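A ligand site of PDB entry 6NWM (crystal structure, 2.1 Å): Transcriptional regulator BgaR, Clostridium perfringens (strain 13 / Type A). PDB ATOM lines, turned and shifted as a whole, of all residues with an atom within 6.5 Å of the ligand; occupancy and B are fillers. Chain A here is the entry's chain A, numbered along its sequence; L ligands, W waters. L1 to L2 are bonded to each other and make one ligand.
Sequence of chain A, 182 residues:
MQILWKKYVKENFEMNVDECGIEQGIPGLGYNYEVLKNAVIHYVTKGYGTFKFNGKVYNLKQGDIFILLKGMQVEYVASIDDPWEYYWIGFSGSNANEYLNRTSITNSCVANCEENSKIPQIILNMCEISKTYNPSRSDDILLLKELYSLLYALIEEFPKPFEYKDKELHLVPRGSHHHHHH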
ATOM      1  N   GLN A   2     -18.042  -5.383 -18.905  1.00  0.00           N
ATOM      2  CA  GLN A   2     -17.051  -4.306 -19.092  1.00  0.00           C
ATOM      3  C   GLN A   2     -17.528  -3.416 -20.241  1.00  0.00           C
ATOM      4  O   GLN A   2     -18.051  -3.987 -21.226  1.00  0.00           O
ATOM      5  CB  GLN A   2     -15.699  -4.934 -19.390  1.00  0.00           C
ATOM      6  CG  GLN A   2     -15.057  -5.578 -18.168  1.00  0.00           C
ATOM      7  CD  GLN A   2     -15.318  -7.060 -18.059  1.00  0.00           C
ATOM      8  OE1 GLN A   2     -15.743  -7.719 -19.007  1.00  0.00           O
ATOM      9  NE2 GLN A   2     -15.053  -7.608 -16.879  1.00  0.00           N
ATOM     10  N   TRP A   5     -13.419  -4.534 -23.446  1.00  0.00           N
ATOM     11  CA  TRP A   5     -12.418  -5.591 -23.143  1.00  0.00           C
ATOM     12  C   TRP A   5     -11.939  -6.194 -24.479  1.00  0.00           C
ATOM     13  O   TRP A   5     -12.452  -7.243 -24.878  1.00  0.00           O
ATOM     14  CB  TRP A   5     -12.941  -6.680 -22.204  1.00  0.00           C
ATOM     15  CG  TRP A   5     -11.836  -7.468 -21.566  1.00  0.00           C
ATOM     16  CD1 TRP A   5     -10.494  -7.358 -21.847  1.00  0.00           C
ATOM     17  CD2 TRP A   5     -11.933  -8.474 -20.532  1.00  0.00           C
ATOM     18  NE1 TRP A   5      -9.772  -8.193 -21.039  1.00  0.00           N
ATOM     19  CE2 TRP A   5     -10.616  -8.894 -20.224  1.00  0.00           C
ATOM     20  CE3 TRP A   5     -12.998  -9.049 -19.828  1.00  0.00           C
ATOM     21  CZ2 TRP A   5     -10.345  -9.860 -19.254  1.00  0.00           C
ATOM     22  CZ3 TRP A   5     -12.725 -10.004 -18.867  1.00  0.00           C
ATOM     23  CH2 TRP A   5     -11.421 -10.405 -18.586  1.00  0.00           C
ATOM     24  N   LYS A   7      -9.280  -8.114 -26.474  1.00  0.00           N
ATOM     25  CA  LYS A   7      -8.129  -9.048 -26.330  1.00  0.00           C
ATOM     26  C   LYS A   7      -7.474  -9.178 -27.713  1.00  0.00           C
ATOM     27  O   LYS A   7      -8.222  -9.358 -28.686  1.00  0.00           O
ATOM     28  CB  LYS A   7      -8.575 -10.394 -25.750  1.00  0.00           C
ATOM     29  CG  LYS A   7      -8.796 -10.387 -24.251  1.00  0.00           C
ATOM     30  CD  LYS A   7      -9.066 -11.784 -23.698  1.00  0.00           C
ATOM     31  CE  LYS A   7      -9.669 -11.795 -22.315  1.00  0.00           C
ATOM     32  NZ  LYS A   7     -11.052 -11.229 -22.292  1.00  0.00           N
ATOM     33  N   GLU A  19      -4.079  -6.549 -24.485  1.00  0.00           N
ATOM     34  CA  GLU A  19      -5.511  -6.180 -24.332  1.00  0.00           C
ATOM     35  C   GLU A  19      -5.594  -4.750 -23.828  1.00  0.00           C
ATOM     36  O   GLU A  19      -4.621  -4.249 -23.222  1.00  0.00           O
ATOM     37  CB  GLU A  19      -6.256  -7.117 -23.358  1.00  0.00           C
ATOM     38  CG  GLU A  19      -5.554  -7.288 -22.017  1.00  0.00           C
ATOM     39  CD  GLU A  19      -6.300  -7.889 -20.822  1.00  0.00           C
ATOM     40  OE1 GLU A  19      -7.484  -8.220 -20.930  1.00  0.00           O
ATOM     41  OE2 GLU A  19      -5.694  -7.955 -19.724  1.00  0.00           O
ATOM     42  N   GLU A  23     -13.460  -0.523 -17.278  1.00  0.00           N
ATOM     43  CA  GLU A  23     -14.448  -1.145 -16.366  1.00  0.00           C
ATOM     44  C   GLU A  23     -14.964  -0.124 -15.351  1.00  0.00           C
ATOM     45  O   GLU A  23     -14.145   0.462 -14.616  1.00  0.00           O
ATOM     46  CB  GLU A  23     -13.894  -2.382 -15.653  1.00  0.00           C
ATOM     47  CG  GLU A  23     -14.951  -3.095 -14.821  1.00  0.00           C
ATOM     48  CD  GLU A  23     -14.626  -4.516 -14.416  1.00  0.00           C
ATOM     49  OE1 GLU A  23     -13.919  -5.206 -15.185  1.00  0.00           O
ATOM     50  OE2 GLU A  23     -15.103  -4.948 -13.339  1.00  0.00           O
ATOM     51  N   TYR A  31     -12.107  -8.274  -7.603  1.00  0.00           N
ATOM     52  CA  TYR A  31     -11.371  -9.457  -8.083  1.00  0.00           C
ATOM     53  C   TYR A  31     -10.300  -9.788  -7.067  1.00  0.00           C
ATOM     54  O   TYR A  31      -9.734  -8.866  -6.465  1.00  0.00           O
ATOM     55  CB  TYR A  31     -10.784  -9.179  -9.480  1.00  0.00           C
ATOM     56  CG  TYR A  31     -11.823  -8.715 -10.450  1.00  0.00           C
ATOM     57  CD1 TYR A  31     -12.703  -9.628 -11.018  1.00  0.00           C
ATOM     58  CD2 TYR A  31     -12.014  -7.374 -10.703  1.00  0.00           C
ATOM     59  CE1 TYR A  31     -13.735  -9.209 -11.842  1.00  0.00           C
ATOM     60  CE2 TYR A  31     -13.023  -6.937 -11.533  1.00  0.00           C
ATOM     61  CZ  TYR A  31     -13.867  -7.859 -12.118  1.00  0.00           C
ATOM     62  OH  TYR A  31     -14.855  -7.436 -12.975  1.00  0.00           O
ATOM     63  N   ASN A  32     -10.052 -11.087  -6.925  1.00  0.00           N
ATOM     64  CA  ASN A  32      -9.074 -11.683  -5.993  1.00  0.00           C
ATOM     65  C   ASN A  32      -8.503 -12.885  -6.722  1.00  0.00           C
ATOM     66  O   ASN A  32      -9.250 -13.844  -6.921  1.00  0.00           O
ATOM     67  CB  ASN A  32      -9.742 -12.045  -4.660  1.00  0.00           C
ATOM     68  CG  ASN A  32      -8.745 -12.504  -3.607  1.00  0.00           C
ATOM     69  OD1 ASN A  32      -7.691 -13.032  -3.936  1.00  0.00           O
ATOM     70  ND2 ASN A  32      -9.063 -12.310  -2.346  1.00  0.00           N
ATOM     71  N   TYR A  33      -7.259 -12.818  -7.196  1.00  0.00           N
ATOM     72  CA  TYR A  33      -6.655 -13.904  -8.011  1.00  0.00           C
ATOM     73  C   TYR A  33      -5.144 -13.720  -8.052  1.00  0.00           C
ATOM     74  O   TYR A  33      -4.639 -12.641  -7.674  1.00  0.00           O
ATOM     75  CB  TYR A  33      -7.319 -13.960  -9.389  1.00  0.00           C
ATOM     76  CG  TYR A  33      -7.097 -12.745 -10.251  1.00  0.00           C
ATOM     77  CD1 TYR A  33      -7.881 -11.606 -10.122  1.00  0.00           C
ATOM     78  CD2 TYR A  33      -6.070 -12.706 -11.180  1.00  0.00           C
ATOM     79  CE1 TYR A  33      -7.655 -10.476 -10.894  1.00  0.00           C
ATOM     80  CE2 TYR A  33      -5.866 -11.603 -11.981  1.00  0.00           C
ATOM     81  CZ  TYR A  33      -6.644 -10.474 -11.839  1.00  0.00           C
ATOM     82  OH  TYR A  33      -6.402  -9.390 -12.635  1.00  0.00           O
ATOM     83  N   GLU A  34      -4.455 -14.785  -8.430  1.00  0.00           N
ATOM     84  CA  GLU A  34      -3.037 -14.773  -8.828  1.00  0.00           C
ATOM     85  C   GLU A  34      -2.959 -14.352 -10.308  1.00  0.00           C
ATOM     86  O   GLU A  34      -3.613 -14.978 -11.156  1.00  0.00           O
ATOM     87  CB  GLU A  34      -2.381 -16.140  -8.609  1.00  0.00           C
ATOM     88  CG  GLU A  34      -0.865 -16.078  -8.720  1.00  0.00           C
ATOM     89  CD  GLU A  34      -0.148 -17.408  -8.751  1.00  0.00           C
ATOM     90  OE1 GLU A  34      -0.033 -18.017  -7.691  1.00  0.00           O
ATOM     91  OE2 GLU A  34       0.312 -17.826  -9.849  1.00  0.00           O
ATOM     92  N   VAL A  35      -2.198 -13.299 -10.583  1.00  0.00           N
ATOM     93  CA  VAL A  35      -2.045 -12.734 -11.956  1.00  0.00           C
ATOM     94  C   VAL A  35      -1.325 -13.782 -12.838  1.00  0.00           C
ATOM     95  O   VAL A  35      -0.222 -14.205 -12.476  1.00  0.00           O
ATOM     96  CB  VAL A  35      -1.293 -11.392 -11.898  1.00  0.00           C
ATOM     97  CG1 VAL A  35      -1.021 -10.843 -13.300  1.00  0.00           C
ATOM     98  CG2 VAL A  35      -2.046 -10.364 -11.050  1.00  0.00           C
ATOM     99  N   LEU A  36      -1.962 -14.143 -13.949  1.00  0.00           N
ATOM    100  CA  LEU A  36      -1.446 -15.037 -15.019  1.00  0.00           C
ATOM    101  C   LEU A  36      -0.843 -14.209 -16.165  1.00  0.00           C
ATOM    102  O   LEU A  36       0.068 -14.706 -16.803  1.00  0.00           O
ATOM    103  CB  LEU A  36      -2.618 -15.882 -15.540  1.00  0.00           C
ATOM    104  CG  LEU A  36      -3.344 -16.702 -14.473  1.00  0.00           C
ATOM    105  CD1 LEU A  36      -4.525 -17.443 -15.083  1.00  0.00           C
ATOM    106  CD2 LEU A  36      -2.388 -17.661 -13.791  1.00  0.00           C
ATOM    107  N   LYS A  37      -1.383 -13.024 -16.449  1.00  0.00           N
ATOM    108  CA  LYS A  37      -0.940 -12.161 -17.585  1.00  0.00           C
ATOM    109  C   LYS A  37       0.421 -11.554 -17.263  1.00  0.00           C
ATOM    110  O   LYS A  37       0.839 -11.564 -16.084  1.00  0.00           O
ATOM    111  CB  LYS A  37      -2.029 -11.149 -17.923  1.00  0.00           C
ATOM    112  CG  LYS A  37      -3.161 -11.785 -18.716  1.00  0.00           C
ATOM    113  CD  LYS A  37      -4.498 -11.137 -18.569  1.00  0.00           C
ATOM    114  CE  LYS A  37      -5.546 -11.883 -19.372  1.00  0.00           C
ATOM    115  NZ  LYS A  37      -6.882 -11.286 -19.223  1.00  0.00           N
ATOM    116  N   VAL A  40      -0.177  -5.678 -16.558  1.00  0.00           N
ATOM    117  CA  VAL A  40      -1.421  -4.935 -16.817  1.00  0.00           C
ATOM    118  C   VAL A  40      -1.405  -3.654 -15.997  1.00  0.00           C
ATOM    119  O   VAL A  40      -1.454  -3.722 -14.778  1.00  0.00           O
ATOM    120  CB  VAL A  40      -2.674  -5.781 -16.544  1.00  0.00           C
ATOM    121  CG1 VAL A  40      -3.889  -5.122 -17.142  1.00  0.00           C
ATOM    122  CG2 VAL A  40      -2.552  -7.221 -17.050  1.00  0.00           C
ATOM    123  N   HIS A  42      -3.234  -0.253 -14.851  1.00  0.00           N
ATOM    124  CA  HIS A  42      -4.577   0.306 -14.596  1.00  0.00           C
ATOM    125  C   HIS A  42      -4.417   1.784 -14.249  1.00  0.00           C
ATOM    126  O   HIS A  42      -3.501   2.125 -13.463  1.00  0.00           O
ATOM    127  CB  HIS A  42      -5.274  -0.465 -13.480  1.00  0.00           C
ATOM    128  CG  HIS A  42      -5.565  -1.889 -13.796  1.00  0.00           C
ATOM    129  ND1 HIS A  42      -4.574  -2.843 -13.853  1.00  0.00           N
ATOM    130  CD2 HIS A  42      -6.726  -2.533 -14.014  1.00  0.00           C
ATOM    131  CE1 HIS A  42      -5.123  -4.003 -14.086  1.00  0.00           C
ATOM    132  NE2 HIS A  42      -6.437  -3.850 -14.202  1.00  0.00           N
ATOM    133  N   PHE A  66      -2.077   1.369 -10.725  1.00  0.00           N
ATOM    134  CA  PHE A  66      -1.581   0.127 -10.093  1.00  0.00           C
ATOM    135  C   PHE A  66      -1.218  -0.799 -11.233  1.00  0.00           C
ATOM    136  O   PHE A  66      -1.876  -0.772 -12.288  1.00  0.00           O
ATOM    137  CB  PHE A  66      -2.595  -0.401  -9.082  1.00  0.00           C
ATOM    138  CG  PHE A  66      -3.939  -0.839  -9.605  1.00  0.00           C
ATOM    139  CD1 PHE A  66      -4.990   0.061  -9.699  1.00  0.00           C
ATOM    140  CD2 PHE A  66      -4.183  -2.165  -9.922  1.00  0.00           C
ATOM    141  CE1 PHE A  66      -6.254  -0.356 -10.126  1.00  0.00           C
ATOM    142  CE2 PHE A  66      -5.434  -2.578 -10.352  1.00  0.00           C
ATOM    143  CZ  PHE A  66      -6.466  -1.683 -10.436  1.00  0.00           C
ATOM    144  N   LEU A  68      -0.357  -4.868 -12.352  1.00  0.00           N
ATOM    145  CA  LEU A  68      -0.408  -6.314 -12.071  1.00  0.00           C
ATOM    146  C   LEU A  68       0.716  -6.951 -12.873  1.00  0.00           C
ATOM    147  O   LEU A  68       0.798  -6.664 -14.086  1.00  0.00           O
ATOM    148  CB  LEU A  68      -1.769  -6.875 -12.511  1.00  0.00           C
ATOM    149  CG  LEU A  68      -2.994  -6.166 -11.949  1.00  0.00           C
ATOM    150  CD1 LEU A  68      -4.247  -6.872 -12.382  1.00  0.00           C
ATOM    151  CD2 LEU A  68      -2.940  -6.046 -10.436  1.00  0.00           C
ATOM    152  N   TYR A  76      -8.479  -6.285  -5.844  1.00  0.00           N
ATOM    153  CA  TYR A  76      -8.832  -4.876  -6.140  1.00  0.00           C
ATOM    154  C   TYR A  76     -10.338  -4.793  -6.227  1.00  0.00           C
ATOM    155  O   TYR A  76     -10.963  -5.602  -6.980  1.00  0.00           O
ATOM    156  CB  TYR A  76      -8.079  -4.325  -7.363  1.00  0.00           C
ATOM    157  CG  TYR A  76      -8.041  -5.167  -8.623  1.00  0.00           C
ATOM    158  CD1 TYR A  76      -7.241  -6.303  -8.719  1.00  0.00           C
ATOM    159  CD2 TYR A  76      -8.740  -4.794  -9.747  1.00  0.00           C
ATOM    160  CE1 TYR A  76      -7.156  -7.029  -9.893  1.00  0.00           C
ATOM    161  CE2 TYR A  76      -8.660  -5.502 -10.920  1.00  0.00           C
ATOM    162  CZ  TYR A  76      -7.899  -6.660 -10.984  1.00  0.00           C
ATOM    163  OH  TYR A  76      -7.811  -7.344 -12.160  1.00  0.00           O
ATOM    164  N   TYR A  86     -11.784   2.375 -14.091  1.00  0.00           N
ATOM    165  CA  TYR A  86     -10.373   2.302 -14.499  1.00  0.00           C
ATOM    166  C   TYR A  86     -10.278   1.860 -15.971  1.00  0.00           C
ATOM    167  O   TYR A  86     -11.217   1.200 -16.520  1.00  0.00           O
ATOM    168  CB  TYR A  86      -9.574   1.472 -13.505  1.00  0.00           C
ATOM    169  CG  TYR A  86     -10.052   0.065 -13.236  1.00  0.00           C
ATOM    170  CD1 TYR A  86     -10.035  -0.909 -14.208  1.00  0.00           C
ATOM    171  CD2 TYR A  86     -10.423  -0.321 -11.961  1.00  0.00           C
ATOM    172  CE1 TYR A  86     -10.425  -2.215 -13.950  1.00  0.00           C
ATOM    173  CE2 TYR A  86     -10.806  -1.627 -11.676  1.00  0.00           C
ATOM    174  CZ  TYR A  86     -10.818  -2.577 -12.671  1.00  0.00           C
ATOM    175  OH  TYR A  86     -11.209  -3.854 -12.384  1.00  0.00           O
ATOM    176  N   TRP A  88      -7.391  -0.001 -18.572  1.00  0.00           N
ATOM    177  CA  TRP A  88      -6.174  -0.843 -18.419  1.00  0.00           C
ATOM    178  C   TRP A  88      -5.592  -1.226 -19.767  1.00  0.00           C
ATOM    179  O   TRP A  88      -6.369  -1.351 -20.757  1.00  0.00           O
ATOM    180  CB  TRP A  88      -6.455  -2.055 -17.542  1.00  0.00           C
ATOM    181  CG  TRP A  88      -7.147  -3.189 -18.237  1.00  0.00           C
ATOM    182  CD1 TRP A  88      -6.592  -4.220 -18.940  1.00  0.00           C
ATOM    183  CD2 TRP A  88      -8.551  -3.434 -18.205  1.00  0.00           C
ATOM    184  NE1 TRP A  88      -7.569  -5.083 -19.377  1.00  0.00           N
ATOM    185  CE2 TRP A  88      -8.777  -4.637 -18.918  1.00  0.00           C
ATOM    186  CE3 TRP A  88      -9.636  -2.779 -17.610  1.00  0.00           C
ATOM    187  CZ2 TRP A  88     -10.059  -5.163 -19.074  1.00  0.00           C
ATOM    188  CZ3 TRP A  88     -10.894  -3.308 -17.765  1.00  0.00           C
ATOM    189  CH2 TRP A  88     -11.111  -4.475 -18.488  1.00  0.00           C
ATOM    190  N   GLY A  90      -2.951  -4.200 -21.066  1.00  0.00           N
ATOM    191  CA  GLY A  90      -2.174  -5.446 -20.883  1.00  0.00           C
ATOM    192  C   GLY A  90      -1.115  -5.549 -21.974  1.00  0.00           C
ATOM    193  O   GLY A  90      -1.448  -5.304 -23.162  1.00  0.00           O
HETATM  194  C1  LIG L   1      -6.901 -13.825 -14.983  1.00  0.00           C
HETATM  195  C2  LIG L   1      -8.225 -13.126 -15.249  1.00  0.00           C
HETATM  196  C3  LIG L   1      -8.216 -11.581 -15.137  1.00  0.00           C
HETATM  197  C4  LIG L   1      -9.670 -11.322 -14.727  1.00  0.00           C
HETATM  198  C5  LIG L   1      -9.836 -12.412 -13.680  1.00  0.00           C
HETATM  199  C6  LIG L   1     -11.262 -12.780 -13.324  1.00  0.00           C
HETATM  200  O1  LIG L   1      -5.868 -13.409 -15.877  1.00  0.00           O
HETATM  201  O2  LIG L   1      -8.656 -13.503 -16.527  1.00  0.00           O
HETATM  202  O3  LIG L   1      -7.806 -10.884 -16.303  1.00  0.00           O
HETATM  203  O4  LIG L   1      -9.859 -10.042 -14.139  1.00  0.00           O
HETATM  204  O5  LIG L   1      -9.151 -13.555 -14.250  1.00  0.00           O
HETATM  205  O6  LIG L   1     -11.306 -13.248 -11.975  1.00  0.00           O
HETATM  206  C1  LG2 L   2      -9.799  -8.937 -15.022  1.00  0.00           C
HETATM  207  C2  LG2 L   2     -10.730  -7.857 -14.475  1.00  0.00           C
HETATM  208  C3  LG2 L   2     -10.600  -6.557 -15.266  1.00  0.00           C
HETATM  209  C4  LG2 L   2      -9.151  -6.135 -15.469  1.00  0.00           C
HETATM  210  C5  LG2 L   2      -8.362  -7.341 -16.041  1.00  0.00           C
HETATM  211  C6  LG2 L   2      -6.878  -7.096 -16.261  1.00  0.00           C
HETATM  212  O1  LG2 L   2     -12.064  -8.360 -14.539  1.00  0.00           O
HETATM  213  O2  LG2 L   2     -11.313  -5.542 -14.574  1.00  0.00           O
HETATM  214  O3  LG2 L   2      -8.622  -5.718 -14.210  1.00  0.00           O
HETATM  215  O4  LG2 L   2      -8.463  -8.449 -15.112  1.00  0.00           O
HETATM  216  O5  LG2 L   2      -6.198  -8.251 -16.837  1.00  0.00           O
HETATM  217  O   HOH W   1      -4.784  -9.637 -14.969  1.00  0.00           O
HETATM  218  O   HOH W   2     -11.552 -12.594  -8.934  1.00  0.00           O
HETATM  219  O   HOH W   3      -5.824 -15.505 -17.694  1.00  0.00           O
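OH of Tyr 86 lies within hydrogen-bond range of O2 of LG2 L2, at 2.8 Å. OH of Tyr 33 is in hydrogen-bond range of O4 of LG2 L2 (3.4 Å). The side-chain hydroxyl of Tyr 76 sits at hydrogen-bond distance from an oxygen (O3) of LG2 L2, 2.7 Å away. The side-chain amino group of Lys 37 lies within hydrogen-bond range of an oxygen (O3) of LIG L1. OE2 of Glu 19 sits at hydrogen-bond distance from O5 of LG2 L2 (2.9 Å). NE2 of His 42 sits at hydrogen-bond distance from O3 of LG2 L2 (2.9 Å). The side-chain hydroxyl of Tyr 31 lies close to an oxygen (O1) of LG2 L2 (3.3 Å). The side-chain carboxylate of Glu 23 lies within hydrogen-bond range of an oxygen (O2) of LG2 L2, at 2.7 Å.
Water W1 lies within hydrogen-bond range of an oxygen (O5) of LG2 L2 (2.7 Å) and the side-chain hydroxyl of Tyr 33 (2.9 Å). Water W2 lies within hydrogen-bond range of N of Asn 32 (2.9 Å) and O6 of LIG L1 (3.1 Å).
Merely in contact with the ligand: Val 40, Trp 88 and Gln 2. Hydrophobic or aromatic side chains within 4 Å of the ligand: Tyr 31, Tyr 33, Val 40, His 42, Tyr 76, Tyr 86 and Trp 88. Of the 20 residues printed, 11 come within 4 Å of the ligand.
The side-chain carboxylate of Glu 23 sits at hydrogen-bond distance from the side-chain hydroxyl of Tyr 31, 2.5 Å away. The backbone NH of Tyr 76 lies within hydrogen-bond range of the backbone carbonyl oxygen of Tyr 31. OE1 of Glu 19 is in salt-bridge range of NZ of Lys 37 (3.6 Å). O of Glu 19 lies within hydrogen-bond range of N of Gly 90, at 2.7 Å. O of Leu 68 lies within hydrogen-bond range of N of Val 40 (2.8 Å). A ring nitrogen (ND1) of His 42 lies within hydrogen-bond range of the backbone carbonyl oxygen (O) of Val 40. The side-chain carboxylate of Glu 19 lies close to the indole nitrogen of Trp 88. NE2 of Gln 2 lies within hydrogen-bond range of OE1 of Glu 23, 3.2 Å away.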
